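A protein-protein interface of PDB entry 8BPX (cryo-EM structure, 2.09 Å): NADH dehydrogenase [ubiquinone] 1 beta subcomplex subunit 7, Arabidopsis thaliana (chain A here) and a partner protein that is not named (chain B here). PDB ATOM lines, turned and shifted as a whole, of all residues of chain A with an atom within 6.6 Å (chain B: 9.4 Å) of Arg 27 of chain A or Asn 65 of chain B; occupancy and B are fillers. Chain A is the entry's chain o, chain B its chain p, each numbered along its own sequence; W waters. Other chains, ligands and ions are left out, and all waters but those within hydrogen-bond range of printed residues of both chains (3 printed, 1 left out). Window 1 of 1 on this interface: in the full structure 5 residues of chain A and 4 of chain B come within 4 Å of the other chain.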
ATOM      1  N   MET A  10     -24.058 -37.370 -13.425  1.00  0.00           N
ATOM      2  CA  MET A  10     -24.857 -36.204 -13.073  1.00  0.00           C
ATOM      3  C   MET A  10     -25.531 -35.610 -14.300  1.00  0.00           C
ATOM      4  O   MET A  10     -24.882 -35.339 -15.313  1.00  0.00           O
ATOM      5  CB  MET A  10     -23.997 -35.152 -12.379  1.00  0.00           C
ATOM      6  CG  MET A  10     -24.824 -34.049 -11.763  1.00  0.00           C
ATOM      7  SD  MET A  10     -25.656 -34.554 -10.247  1.00  0.00           S
ATOM      8  CE  MET A  10     -26.707 -33.132  -9.974  1.00  0.00           C
ATOM      9  N   GLN A  14     -25.836 -27.241 -12.197  1.00  0.00           N
ATOM     10  CA  GLN A  14     -25.885 -26.400 -11.009  1.00  0.00           C
ATOM     11  C   GLN A  14     -26.957 -25.328 -11.142  1.00  0.00           C
ATOM     12  O   GLN A  14     -27.686 -25.040 -10.184  1.00  0.00           O
ATOM     13  CB  GLN A  14     -24.522 -25.765 -10.759  1.00  0.00           C
ATOM     14  CG  GLN A  14     -23.596 -26.614  -9.934  1.00  0.00           C
ATOM     15  CD  GLN A  14     -22.138 -26.430 -10.296  1.00  0.00           C
ATOM     16  OE1 GLN A  14     -21.787 -26.273 -11.461  1.00  0.00           O
ATOM     17  NE2 GLN A  14     -21.280 -26.424  -9.284  1.00  0.00           N
ATOM     18  N   MET A  17     -30.482 -26.793 -10.514  1.00  0.00           N
ATOM     19  CA  MET A  17     -30.727 -27.093  -9.109  1.00  0.00           C
ATOM     20  C   MET A  17     -30.911 -25.820  -8.292  1.00  0.00           C
ATOM     21  O   MET A  17     -31.731 -25.790  -7.368  1.00  0.00           O
ATOM     22  CB  MET A  17     -29.592 -27.946  -8.544  1.00  0.00           C
ATOM     23  CG  MET A  17     -29.652 -29.392  -9.015  1.00  0.00           C
ATOM     24  SD  MET A  17     -28.440 -30.470  -8.244  1.00  0.00           S
ATOM     25  CE  MET A  17     -26.917 -29.678  -8.734  1.00  0.00           C
ATOM     26  N   SER A  18     -30.161 -24.761  -8.615  1.00  0.00           N
ATOM     27  CA  SER A  18     -30.347 -23.487  -7.924  1.00  0.00           C
ATOM     28  C   SER A  18     -31.685 -22.847  -8.282  1.00  0.00           C
ATOM     29  O   SER A  18     -32.357 -22.279  -7.414  1.00  0.00           O
ATOM     30  CB  SER A  18     -29.201 -22.532  -8.252  1.00  0.00           C
ATOM     31  OG  SER A  18     -28.023 -22.884  -7.559  1.00  0.00           O
ATOM     32  N   ALA A  19     -32.078 -22.911  -9.557  1.00  0.00           N
ATOM     33  CA  ALA A  19     -33.353 -22.338  -9.970  1.00  0.00           C
ATOM     34  C   ALA A  19     -34.528 -23.063  -9.337  1.00  0.00           C
ATOM     35  O   ALA A  19     -35.521 -22.427  -8.973  1.00  0.00           O
ATOM     36  CB  ALA A  19     -33.480 -22.361 -11.491  1.00  0.00           C
ATOM     37  N   ALA A  20     -34.442 -24.385  -9.207  1.00  0.00           N
ATOM     38  CA  ALA A  20     -35.491 -25.154  -8.552  1.00  0.00           C
ATOM     39  C   ALA A  20     -35.433 -25.055  -7.033  1.00  0.00           C
ATOM     40  O   ALA A  20     -36.285 -25.646  -6.362  1.00  0.00           O
ATOM     41  CB  ALA A  20     -35.419 -26.621  -8.980  1.00  0.00           C
ATOM     42  N   LYS A  21     -34.472 -24.398  -6.445  1.00  0.00           N
ATOM     43  CA  LYS A  21     -34.275 -24.229  -4.959  1.00  0.00           C
ATOM     44  C   LYS A  21     -34.213 -25.561  -4.210  1.00  0.00           C
ATOM     45  O   LYS A  21     -34.834 -25.639  -3.193  1.00  0.00           O
ATOM     46  CB  LYS A  21     -35.295 -23.203  -4.434  1.00  0.00           C
ATOM     47  CG  LYS A  21     -34.891 -21.760  -4.684  1.00  0.00           C
ATOM     48  CD  LYS A  21     -36.019 -20.833  -5.037  1.00  0.00           C
ATOM     49  CE  LYS A  21     -36.814 -20.354  -3.848  1.00  0.00           C
ATOM     50  NZ  LYS A  21     -37.370 -19.000  -4.081  1.00  0.00           N
ATOM     51  N   ILE A  22     -33.397 -26.503  -4.674  1.00  0.00           N
ATOM     52  CA  ILE A  22     -33.218 -27.798  -3.977  1.00  0.00           C
ATOM     53  C   ILE A  22     -32.389 -27.622  -2.707  1.00  0.00           C
ATOM     54  O   ILE A  22     -31.353 -27.057  -2.797  1.00  0.00           O
ATOM     55  CB  ILE A  22     -32.546 -28.869  -4.891  1.00  0.00           C
ATOM     56  CG1 ILE A  22     -33.094 -28.860  -6.324  1.00  0.00           C
ATOM     57  CG2 ILE A  22     -32.606 -30.234  -4.257  1.00  0.00           C
ATOM     58  CD1 ILE A  22     -34.571 -29.096  -6.429  1.00  0.00           C
ATOM     59  N   ALA A  23     -32.868 -28.162  -1.603  1.00  0.00           N
ATOM     60  CA  ALA A  23     -32.108 -28.250  -0.358  1.00  0.00           C
ATOM     61  C   ALA A  23     -30.767 -28.868  -0.716  1.00  0.00           C
ATOM     62  O   ALA A  23     -30.748 -29.870  -1.491  1.00  0.00           O
ATOM     63  CB  ALA A  23     -32.896 -29.111   0.576  1.00  0.00           C
ATOM     64  N   LEU A  24     -29.686 -28.337  -0.170  1.00  0.00           N
ATOM     65  CA  LEU A  24     -28.336 -28.746  -0.566  1.00  0.00           C
ATOM     66  C   LEU A  24     -28.147 -30.264  -0.468  1.00  0.00           C
ATOM     67  O   LEU A  24     -27.457 -30.762  -1.309  1.00  0.00           O
ATOM     68  CB  LEU A  24     -27.350 -27.965   0.316  1.00  0.00           C
ATOM     69  CG  LEU A  24     -27.335 -26.449   0.100  1.00  0.00           C
ATOM     70  CD1 LEU A  24     -26.286 -25.784   0.971  1.00  0.00           C
ATOM     71  CD2 LEU A  24     -27.143 -26.061  -1.363  1.00  0.00           C
ATOM     72  N   GLY A  25     -28.689 -30.925   0.567  1.00  0.00           N
ATOM     73  CA  GLY A  25     -28.585 -32.363   0.749  1.00  0.00           C
ATOM     74  C   GLY A  25     -29.366 -33.200  -0.244  1.00  0.00           C
ATOM     75  O   GLY A  25     -29.201 -34.351  -0.219  1.00  0.00           O
ATOM     76  N   SER A  26     -30.185 -32.612  -1.061  1.00  0.00           N
ATOM     77  CA  SER A  26     -30.913 -33.327  -2.142  1.00  0.00           C
ATOM     78  C   SER A  26     -30.332 -32.861  -3.496  1.00  0.00           C
ATOM     79  O   SER A  26     -31.048 -32.883  -4.462  1.00  0.00           O
ATOM     80  CB  SER A  26     -32.368 -33.129  -1.943  1.00  0.00           C
ATOM     81  OG  SER A  26     -32.814 -33.686  -0.737  1.00  0.00           O
ATOM     82  N   ARG A  27     -29.075 -32.416  -3.532  1.00  0.00           N
ATOM     83  CA  ARG A  27     -28.401 -32.082  -4.825  1.00  0.00           C
ATOM     84  C   ARG A  27     -27.470 -33.250  -5.222  1.00  0.00           C
ATOM     85  O   ARG A  27     -26.307 -33.045  -5.360  1.00  0.00           O
ATOM     86  CB  ARG A  27     -27.783 -30.678  -4.801  1.00  0.00           C
ATOM     87  CG  ARG A  27     -28.753 -29.537  -4.567  1.00  0.00           C
ATOM     88  CD  ARG A  27     -28.112 -28.181  -4.754  1.00  0.00           C
ATOM     89  NE  ARG A  27     -29.151 -27.180  -4.663  1.00  0.00           N
ATOM     90  CZ  ARG A  27     -29.004 -25.872  -4.837  1.00  0.00           C
ATOM     91  NH1 ARG A  27     -27.832 -25.352  -5.132  1.00  0.00           N
ATOM     92  NH2 ARG A  27     -30.051 -25.085  -4.720  1.00  0.00           N
ATOM     93  N   ASP A  28     -28.030 -34.408  -5.305  1.00  0.00           N
ATOM     94  CA  ASP A  28     -27.253 -35.599  -5.608  1.00  0.00           C
ATOM     95  C   ASP A  28     -27.511 -36.002  -7.081  1.00  0.00           C
ATOM     96  O   ASP A  28     -28.084 -35.232  -7.807  1.00  0.00           O
ATOM     97  CB  ASP A  28     -27.556 -36.623  -4.519  1.00  0.00           C
ATOM     98  CG  ASP A  28     -28.969 -37.149  -4.416  1.00  0.00           C
ATOM     99  OD1 ASP A  28     -29.281 -37.668  -3.345  1.00  0.00           O
ATOM    100  OD2 ASP A  28     -29.729 -37.048  -5.383  1.00  0.00           O
ATOM    101  N   MET A  29     -27.162 -37.224  -7.436  1.00  0.00           N
ATOM    102  CA  MET A  29     -27.345 -37.665  -8.816  1.00  0.00           C
ATOM    103  C   MET A  29     -28.809 -37.761  -9.226  1.00  0.00           C
ATOM    104  O   MET A  29     -29.097 -37.826 -10.424  1.00  0.00           O
ATOM    105  CB  MET A  29     -26.686 -39.030  -9.024  1.00  0.00           C
ATOM    106  CG  MET A  29     -25.190 -39.041  -8.844  1.00  0.00           C
ATOM    107  SD  MET A  29     -24.285 -38.784 -10.376  1.00  0.00           S
ATOM    108  CE  MET A  29     -23.127 -37.526  -9.858  1.00  0.00           C
ATOM    109  N   CYS A  30     -29.739 -37.762  -8.275  1.00  0.00           N
ATOM    110  CA  CYS A  30     -31.146 -37.992  -8.567  1.00  0.00           C
ATOM    111  C   CYS A  30     -31.953 -36.703  -8.654  1.00  0.00           C
ATOM    112  O   CYS A  30     -33.186 -36.759  -8.662  1.00  0.00           O
ATOM    113  CB  CYS A  30     -31.751 -38.917  -7.509  1.00  0.00           C
ATOM    114  SG  CYS A  30     -31.161 -40.618  -7.557  1.00  0.00           S
ATOM    115  N   ALA A  31     -31.290 -35.546  -8.729  1.00  0.00           N
ATOM    116  CA  ALA A  31     -31.993 -34.268  -8.655  1.00  0.00           C
ATOM    117  C   ALA A  31     -32.777 -33.962  -9.924  1.00  0.00           C
ATOM    118  O   ALA A  31     -33.800 -33.264  -9.865  1.00  0.00           O
ATOM    119  CB  ALA A  31     -30.998 -33.142  -8.361  1.00  0.00           C
ATOM    120  N   LEU A  34     -35.884 -35.092  -8.943  1.00  0.00           N
ATOM    121  CA  LEU A  34     -36.469 -34.328  -7.844  1.00  0.00           C
ATOM    122  C   LEU A  34     -37.175 -33.080  -8.351  1.00  0.00           C
ATOM    123  O   LEU A  34     -38.238 -32.716  -7.839  1.00  0.00           O
ATOM    124  CB  LEU A  34     -35.395 -33.957  -6.817  1.00  0.00           C
ATOM    125  CG  LEU A  34     -35.896 -33.284  -5.527  1.00  0.00           C
ATOM    126  CD1 LEU A  34     -37.077 -34.026  -4.912  1.00  0.00           C
ATOM    127  CD2 LEU A  34     -34.772 -33.130  -4.515  1.00  0.00           C
ATOM    128  N   CYS B  58     -30.270 -10.722   1.255  1.00  0.00           N
ATOM    129  CA  CYS B  58     -29.745 -11.795   0.370  1.00  0.00           C
ATOM    130  C   CYS B  58     -30.170 -13.159   0.937  1.00  0.00           C
ATOM    131  O   CYS B  58     -30.801 -13.859   0.193  1.00  0.00           O
ATOM    132  CB  CYS B  58     -28.263 -11.577   0.088  1.00  0.00           C
ATOM    133  SG  CYS B  58     -27.476 -12.785  -1.000  1.00  0.00           S
ATOM    134  N   TYR B  59     -29.955 -13.440   2.228  1.00  0.00           N
ATOM    135  CA  TYR B  59     -30.472 -14.638   2.905  1.00  0.00           C
ATOM    136  C   TYR B  59     -31.944 -14.809   2.554  1.00  0.00           C
ATOM    137  O   TYR B  59     -32.243 -15.883   2.105  1.00  0.00           O
ATOM    138  CB  TYR B  59     -30.208 -14.667   4.425  1.00  0.00           C
ATOM    139  CG  TYR B  59     -30.523 -15.937   5.145  1.00  0.00           C
ATOM    140  CD1 TYR B  59     -29.568 -16.931   5.245  1.00  0.00           C
ATOM    141  CD2 TYR B  59     -31.755 -16.125   5.743  1.00  0.00           C
ATOM    142  CE1 TYR B  59     -29.832 -18.095   5.922  1.00  0.00           C
ATOM    143  CE2 TYR B  59     -32.034 -17.289   6.430  1.00  0.00           C
ATOM    144  CZ  TYR B  59     -31.068 -18.273   6.512  1.00  0.00           C
ATOM    145  OH  TYR B  59     -31.295 -19.432   7.169  1.00  0.00           O
ATOM    146  N   ARG B  60     -32.761 -13.798   2.794  1.00  0.00           N
ATOM    147  CA  ARG B  60     -34.207 -13.821   2.580  1.00  0.00           C
ATOM    148  C   ARG B  60     -34.554 -14.000   1.099  1.00  0.00           C
ATOM    149  O   ARG B  60     -35.512 -14.628   0.816  1.00  0.00           O
ATOM    150  CB  ARG B  60     -34.829 -12.531   3.130  1.00  0.00           C
ATOM    151  CG  ARG B  60     -34.861 -12.463   4.650  1.00  0.00           C
ATOM    152  CD  ARG B  60     -35.183 -11.115   5.243  1.00  0.00           C
ATOM    153  NE  ARG B  60     -35.158 -11.193   6.693  1.00  0.00           N
ATOM    154  CZ  ARG B  60     -35.641 -10.273   7.514  1.00  0.00           C
ATOM    155  NH1 ARG B  60     -36.188  -9.170   7.045  1.00  0.00           N
ATOM    156  NH2 ARG B  60     -35.569 -10.466   8.811  1.00  0.00           N
ATOM    157  N   VAL B  61     -33.816 -13.325   0.241  1.00  0.00           N
ATOM    158  CA  VAL B  61     -34.230 -13.433  -1.152  1.00  0.00           C
ATOM    159  C   VAL B  61     -33.730 -14.733  -1.774  1.00  0.00           C
ATOM    160  O   VAL B  61     -34.452 -15.388  -2.529  1.00  0.00           O
ATOM    161  CB  VAL B  61     -33.761 -12.194  -1.939  1.00  0.00           C
ATOM    162  CG1 VAL B  61     -33.720 -12.473  -3.435  1.00  0.00           C
ATOM    163  CG2 VAL B  61     -34.668 -11.007  -1.648  1.00  0.00           C
ATOM    164  N   GLU B  62     -32.506 -15.147  -1.458  1.00  0.00           N
ATOM    165  CA  GLU B  62     -31.891 -16.272  -2.149  1.00  0.00           C
ATOM    166  C   GLU B  62     -32.198 -17.632  -1.535  1.00  0.00           C
ATOM    167  O   GLU B  62     -31.929 -18.649  -2.179  1.00  0.00           O
ATOM    168  CB  GLU B  62     -30.377 -16.075  -2.223  1.00  0.00           C
ATOM    169  CG  GLU B  62     -29.970 -14.756  -2.842  1.00  0.00           C
ATOM    170  CD  GLU B  62     -30.161 -14.714  -4.349  1.00  0.00           C
ATOM    171  OE1 GLU B  62     -30.800 -15.620  -4.911  1.00  0.00           O
ATOM    172  OE2 GLU B  62     -29.669 -13.758  -4.976  1.00  0.00           O
ATOM    173  N   GLY B  63     -32.747 -17.677  -0.324  1.00  0.00           N
ATOM    174  CA  GLY B  63     -33.140 -18.947   0.267  1.00  0.00           C
ATOM    175  C   GLY B  63     -31.976 -19.910   0.403  1.00  0.00           C
ATOM    176  O   GLY B  63     -30.914 -19.570   0.927  1.00  0.00           O
ATOM    177  N   VAL B  64     -32.171 -21.173   0.068  1.00  0.00           N
ATOM    178  CA  VAL B  64     -31.107 -22.231   0.037  1.00  0.00           C
ATOM    179  C   VAL B  64     -29.907 -21.893  -0.860  1.00  0.00           C
ATOM    180  O   VAL B  64     -28.900 -22.507  -0.639  1.00  0.00           O
ATOM    181  CB  VAL B  64     -31.724 -23.609  -0.331  1.00  0.00           C
ATOM    182  CG1 VAL B  64     -32.750 -24.062   0.704  1.00  0.00           C
ATOM    183  CG2 VAL B  64     -32.324 -23.606  -1.733  1.00  0.00           C
ATOM    184  N   ASN B  65     -29.981 -20.922  -1.745  1.00  0.00           N
ATOM    185  CA  ASN B  65     -28.816 -20.511  -2.517  1.00  0.00           C
ATOM    186  C   ASN B  65     -28.011 -19.409  -1.831  1.00  0.00           C
ATOM    187  O   ASN B  65     -27.086 -18.860  -2.439  1.00  0.00           O
ATOM    188  CB  ASN B  65     -29.237 -20.052  -3.918  1.00  0.00           C
ATOM    189  CG  ASN B  65     -30.046 -21.101  -4.662  1.00  0.00           C
ATOM    190  OD1 ASN B  65     -29.717 -22.283  -4.645  1.00  0.00           O
ATOM    191  ND2 ASN B  65     -31.108 -20.669  -5.319  1.00  0.00           N
ATOM    192  N   HIS B  66     -28.337 -19.085  -0.576  1.00  0.00           N
ATOM    193  CA  HIS B  66     -27.683 -17.971   0.105  1.00  0.00           C
ATOM    194  C   HIS B  66     -26.189 -18.211   0.303  1.00  0.00           C
ATOM    195  O   HIS B  66     -25.408 -17.260   0.264  1.00  0.00           O
ATOM    196  CB  HIS B  66     -28.369 -17.702   1.446  1.00  0.00           C
ATOM    197  CG  HIS B  66     -27.992 -18.667   2.523  1.00  0.00           C
ATOM    198  ND1 HIS B  66     -26.848 -18.534   3.275  1.00  0.00           N
ATOM    199  CD2 HIS B  66     -28.617 -19.774   2.985  1.00  0.00           C
ATOM    200  CE1 HIS B  66     -26.778 -19.522   4.145  1.00  0.00           C
ATOM    201  NE2 HIS B  66     -27.840 -20.288   3.992  1.00  0.00           N
ATOM    202  N   TYR B  67     -25.776 -19.465   0.505  1.00  0.00           N
ATOM    203  CA  TYR B  67     -24.362 -19.750   0.732  1.00  0.00           C
ATOM    204  C   TYR B  67     -23.508 -19.282  -0.436  1.00  0.00           C
ATOM    205  O   TYR B  67     -22.436 -18.698  -0.241  1.00  0.00           O
ATOM    206  CB  TYR B  67     -24.148 -21.245   0.954  1.00  0.00           C
ATOM    207  CG  TYR B  67     -24.464 -21.752   2.340  1.00  0.00           C
ATOM    208  CD1 TYR B  67     -23.846 -21.215   3.464  1.00  0.00           C
ATOM    209  CD2 TYR B  67     -25.367 -22.786   2.521  1.00  0.00           C
ATOM    210  CE1 TYR B  67     -24.134 -21.693   4.730  1.00  0.00           C
ATOM    211  CE2 TYR B  67     -25.658 -23.271   3.771  1.00  0.00           C
ATOM    212  CZ  TYR B  67     -25.043 -22.724   4.872  1.00  0.00           C
ATOM    213  OH  TYR B  67     -25.343 -23.215   6.118  1.00  0.00           O
ATOM    214  N   GLN B  68     -23.961 -19.533  -1.661  1.00  0.00           N
ATOM    215  CA  GLN B  68     -23.209 -19.134  -2.838  1.00  0.00           C
ATOM    216  C   GLN B  68     -23.516 -17.707  -3.265  1.00  0.00           C
ATOM    217  O   GLN B  68     -22.642 -17.035  -3.817  1.00  0.00           O
ATOM    218  CB  GLN B  68     -23.479 -20.126  -3.981  1.00  0.00           C
ATOM    219  CG  GLN B  68     -23.474 -19.558  -5.388  1.00  0.00           C
ATOM    220  CD  GLN B  68     -23.583 -20.646  -6.445  1.00  0.00           C
ATOM    221  OE1 GLN B  68     -24.464 -21.504  -6.384  1.00  0.00           O
ATOM    222  NE2 GLN B  68     -22.678 -20.621  -7.415  1.00  0.00           N
ATOM    223  N   LYS B  69     -24.717 -17.203  -2.978  1.00  0.00           N
ATOM    224  CA  LYS B  69     -25.065 -15.849  -3.389  1.00  0.00           C
ATOM    225  C   LYS B  69     -24.638 -14.773  -2.392  1.00  0.00           C
ATOM    226  O   LYS B  69     -24.280 -13.671  -2.816  1.00  0.00           O
ATOM    227  CB  LYS B  69     -26.570 -15.740  -3.642  1.00  0.00           C
ATOM    228  CG  LYS B  69     -27.078 -16.656  -4.747  1.00  0.00           C
ATOM    229  CD  LYS B  69     -26.477 -16.285  -6.090  1.00  0.00           C
ATOM    230  CE  LYS B  69     -27.022 -17.138  -7.222  1.00  0.00           C
ATOM    231  NZ  LYS B  69     -26.418 -16.795  -8.541  1.00  0.00           N
ATOM    232  N   CYS B  70     -24.667 -15.049  -1.087  1.00  0.00           N
ATOM    233  CA  CYS B  70     -24.323 -14.051  -0.075  1.00  0.00           C
ATOM    234  C   CYS B  70     -22.839 -13.997   0.245  1.00  0.00           C
ATOM    235  O   CYS B  70     -22.437 -13.180   1.077  1.00  0.00           O
ATOM    236  CB  CYS B  70     -25.072 -14.311   1.243  1.00  0.00           C
ATOM    237  SG  CYS B  70     -26.828 -14.644   1.150  1.00  0.00           S
ATOM    238  N   ARG B  71     -22.024 -14.839  -0.393  1.00  0.00           N
ATOM    239  CA  ARG B  71     -20.658 -15.071   0.068  1.00  0.00           C
ATOM    240  C   ARG B  71     -19.860 -13.773   0.157  1.00  0.00           C
ATOM    241  O   ARG B  71     -19.219 -13.495   1.178  1.00  0.00           O
ATOM    242  CB  ARG B  71     -19.982 -16.072  -0.865  1.00  0.00           C
ATOM    243  CG  ARG B  71     -18.508 -16.236  -0.675  1.00  0.00           C
ATOM    244  CD  ARG B  71     -18.049 -17.538  -1.300  1.00  0.00           C
ATOM    245  NE  ARG B  71     -16.930 -18.127  -0.580  1.00  0.00           N
ATOM    246  CZ  ARG B  71     -15.658 -17.868  -0.850  1.00  0.00           C
ATOM    247  NH1 ARG B  71     -15.315 -17.019  -1.804  1.00  0.00           N
ATOM    248  NH2 ARG B  71     -14.711 -18.480  -0.149  1.00  0.00           N
HETATM  249  O   HOH W   1     -27.582 -20.144  -6.671  1.00  0.00           O
HETATM  250  O   HOH W   2     -26.465 -22.502  -4.661  1.00  0.00           O
HETATM  251  O   HOH W   3     -35.053 -18.160  -2.381  1.00  0.00           O
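Of the printed residues of chain B, Lys 21 of chain A touches Val 64 (3.5 Å) and Asn 65 (3.99 Å).
No residue of chain B comes within 4 Å of Gly 25 of chain A.
No residue of chain B comes within 4 Å of Ser 26 of chain A.
Arg 27 of chain A touches just one residue of chain B: Asn 65 (2.8 Å).
Cys 30 of chain A touches none of the printed residues of chain B.
Printed residues of chain A within 4 Å of Asn 65 of chain B: Ser 18 (2.9 Å), Lys 21 (3.99 Å) and Arg 27 (2.8 Å).
Of the printed residues of chain A, Gln 68 of chain B touches Ser 18 (3.99 Å).
Lys 69 of chain B touches none of the printed residues of chain A.
The nearest printed residue of chain A that does not touch Asn 65 of chain B is Met 17 of chain A (4.9 Å).
The nearest printed residue of chain B that does not touch Lys 21 of chain A is Val 61 of chain B (4.9 Å).
Water W2 lies within hydrogen-bond range of OE1 of Gln 68 of chain B (2.8 Å), NH1 of Arg 27 of chain A (3.2 Å), OD1 of Asn 65 of chain B (3.3 Å) and OG of Ser 18 of chain A (3.3 Å).
Water W3 lies within hydrogen-bond range of the backbone carbonyl oxygen (O) of Val 61 of chain B, the side-chain amino group (NZ) of Lys 21 of chain A, the backbone NH (N) of Gly 63 of chain B and the backbone carbonyl oxygen (O) of Glu 62 of chain B.
Water W1 bridges OG of Ser 18 of chain A and OE1 of Gln 68 of chain B.
NH1 of Arg 27 of chain A is in hydrogen-bond range of OG of Ser 18 of chain A (3.5 Å).
The guanidinium group (NH2) of Arg 27 of chain A is in hydrogen-bond range of the backbone carbonyl oxygen (O) of Met 17 of chain A.
O of Ile 22 of chain A lies within hydrogen-bond range of NE of Arg 27 of chain A, 2.9 Å away.
OG of Ser 18 of chain A lies within hydrogen-bond range of O of Gln 14 of chain A, 3.4 Å away.
O of Met 17 of chain A sits at hydrogen-bond distance from N of Ile 22 of chain A (3.2 Å).
OE1 of Gln 68 of chain B touches OG of Ser 18 of chain A (3.99 Å).
Lys 21 of chain A touches Val 64 of chain B (O to CG2, 3.5 Å).
CG of Lys 21 of chain A touches ND2 of Asn 65 of chain B (3.99 Å).
Val 64 of chain B touches Ile 22 of chain A (CG2 to O, 3.7 Å).
CD1 of Leu 24 of chain A touches CD2 of Tyr 67 of chain B, 3.5 Å away.
The side-chain amide nitrogen (ND2) of Asn 65 of chain B is in hydrogen-bond range of the backbone carbonyl oxygen (O) of Ser 18 of chain A, at 2.9 Å.
The guanidinium group of Arg 27 of chain A sits at hydrogen-bond distance from the side-chain amide oxygen of Asn 65 of chain B (2.8 Å).
Printed residues of chain A that touch a printed residue of chain B: Ser 18, Lys 21, Ile 22, Leu 24 and Arg 27.
Hydrophobic or aromatic side chains of chain B within 4 Å of the printed part of chain A: Val 64 and Tyr 67.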
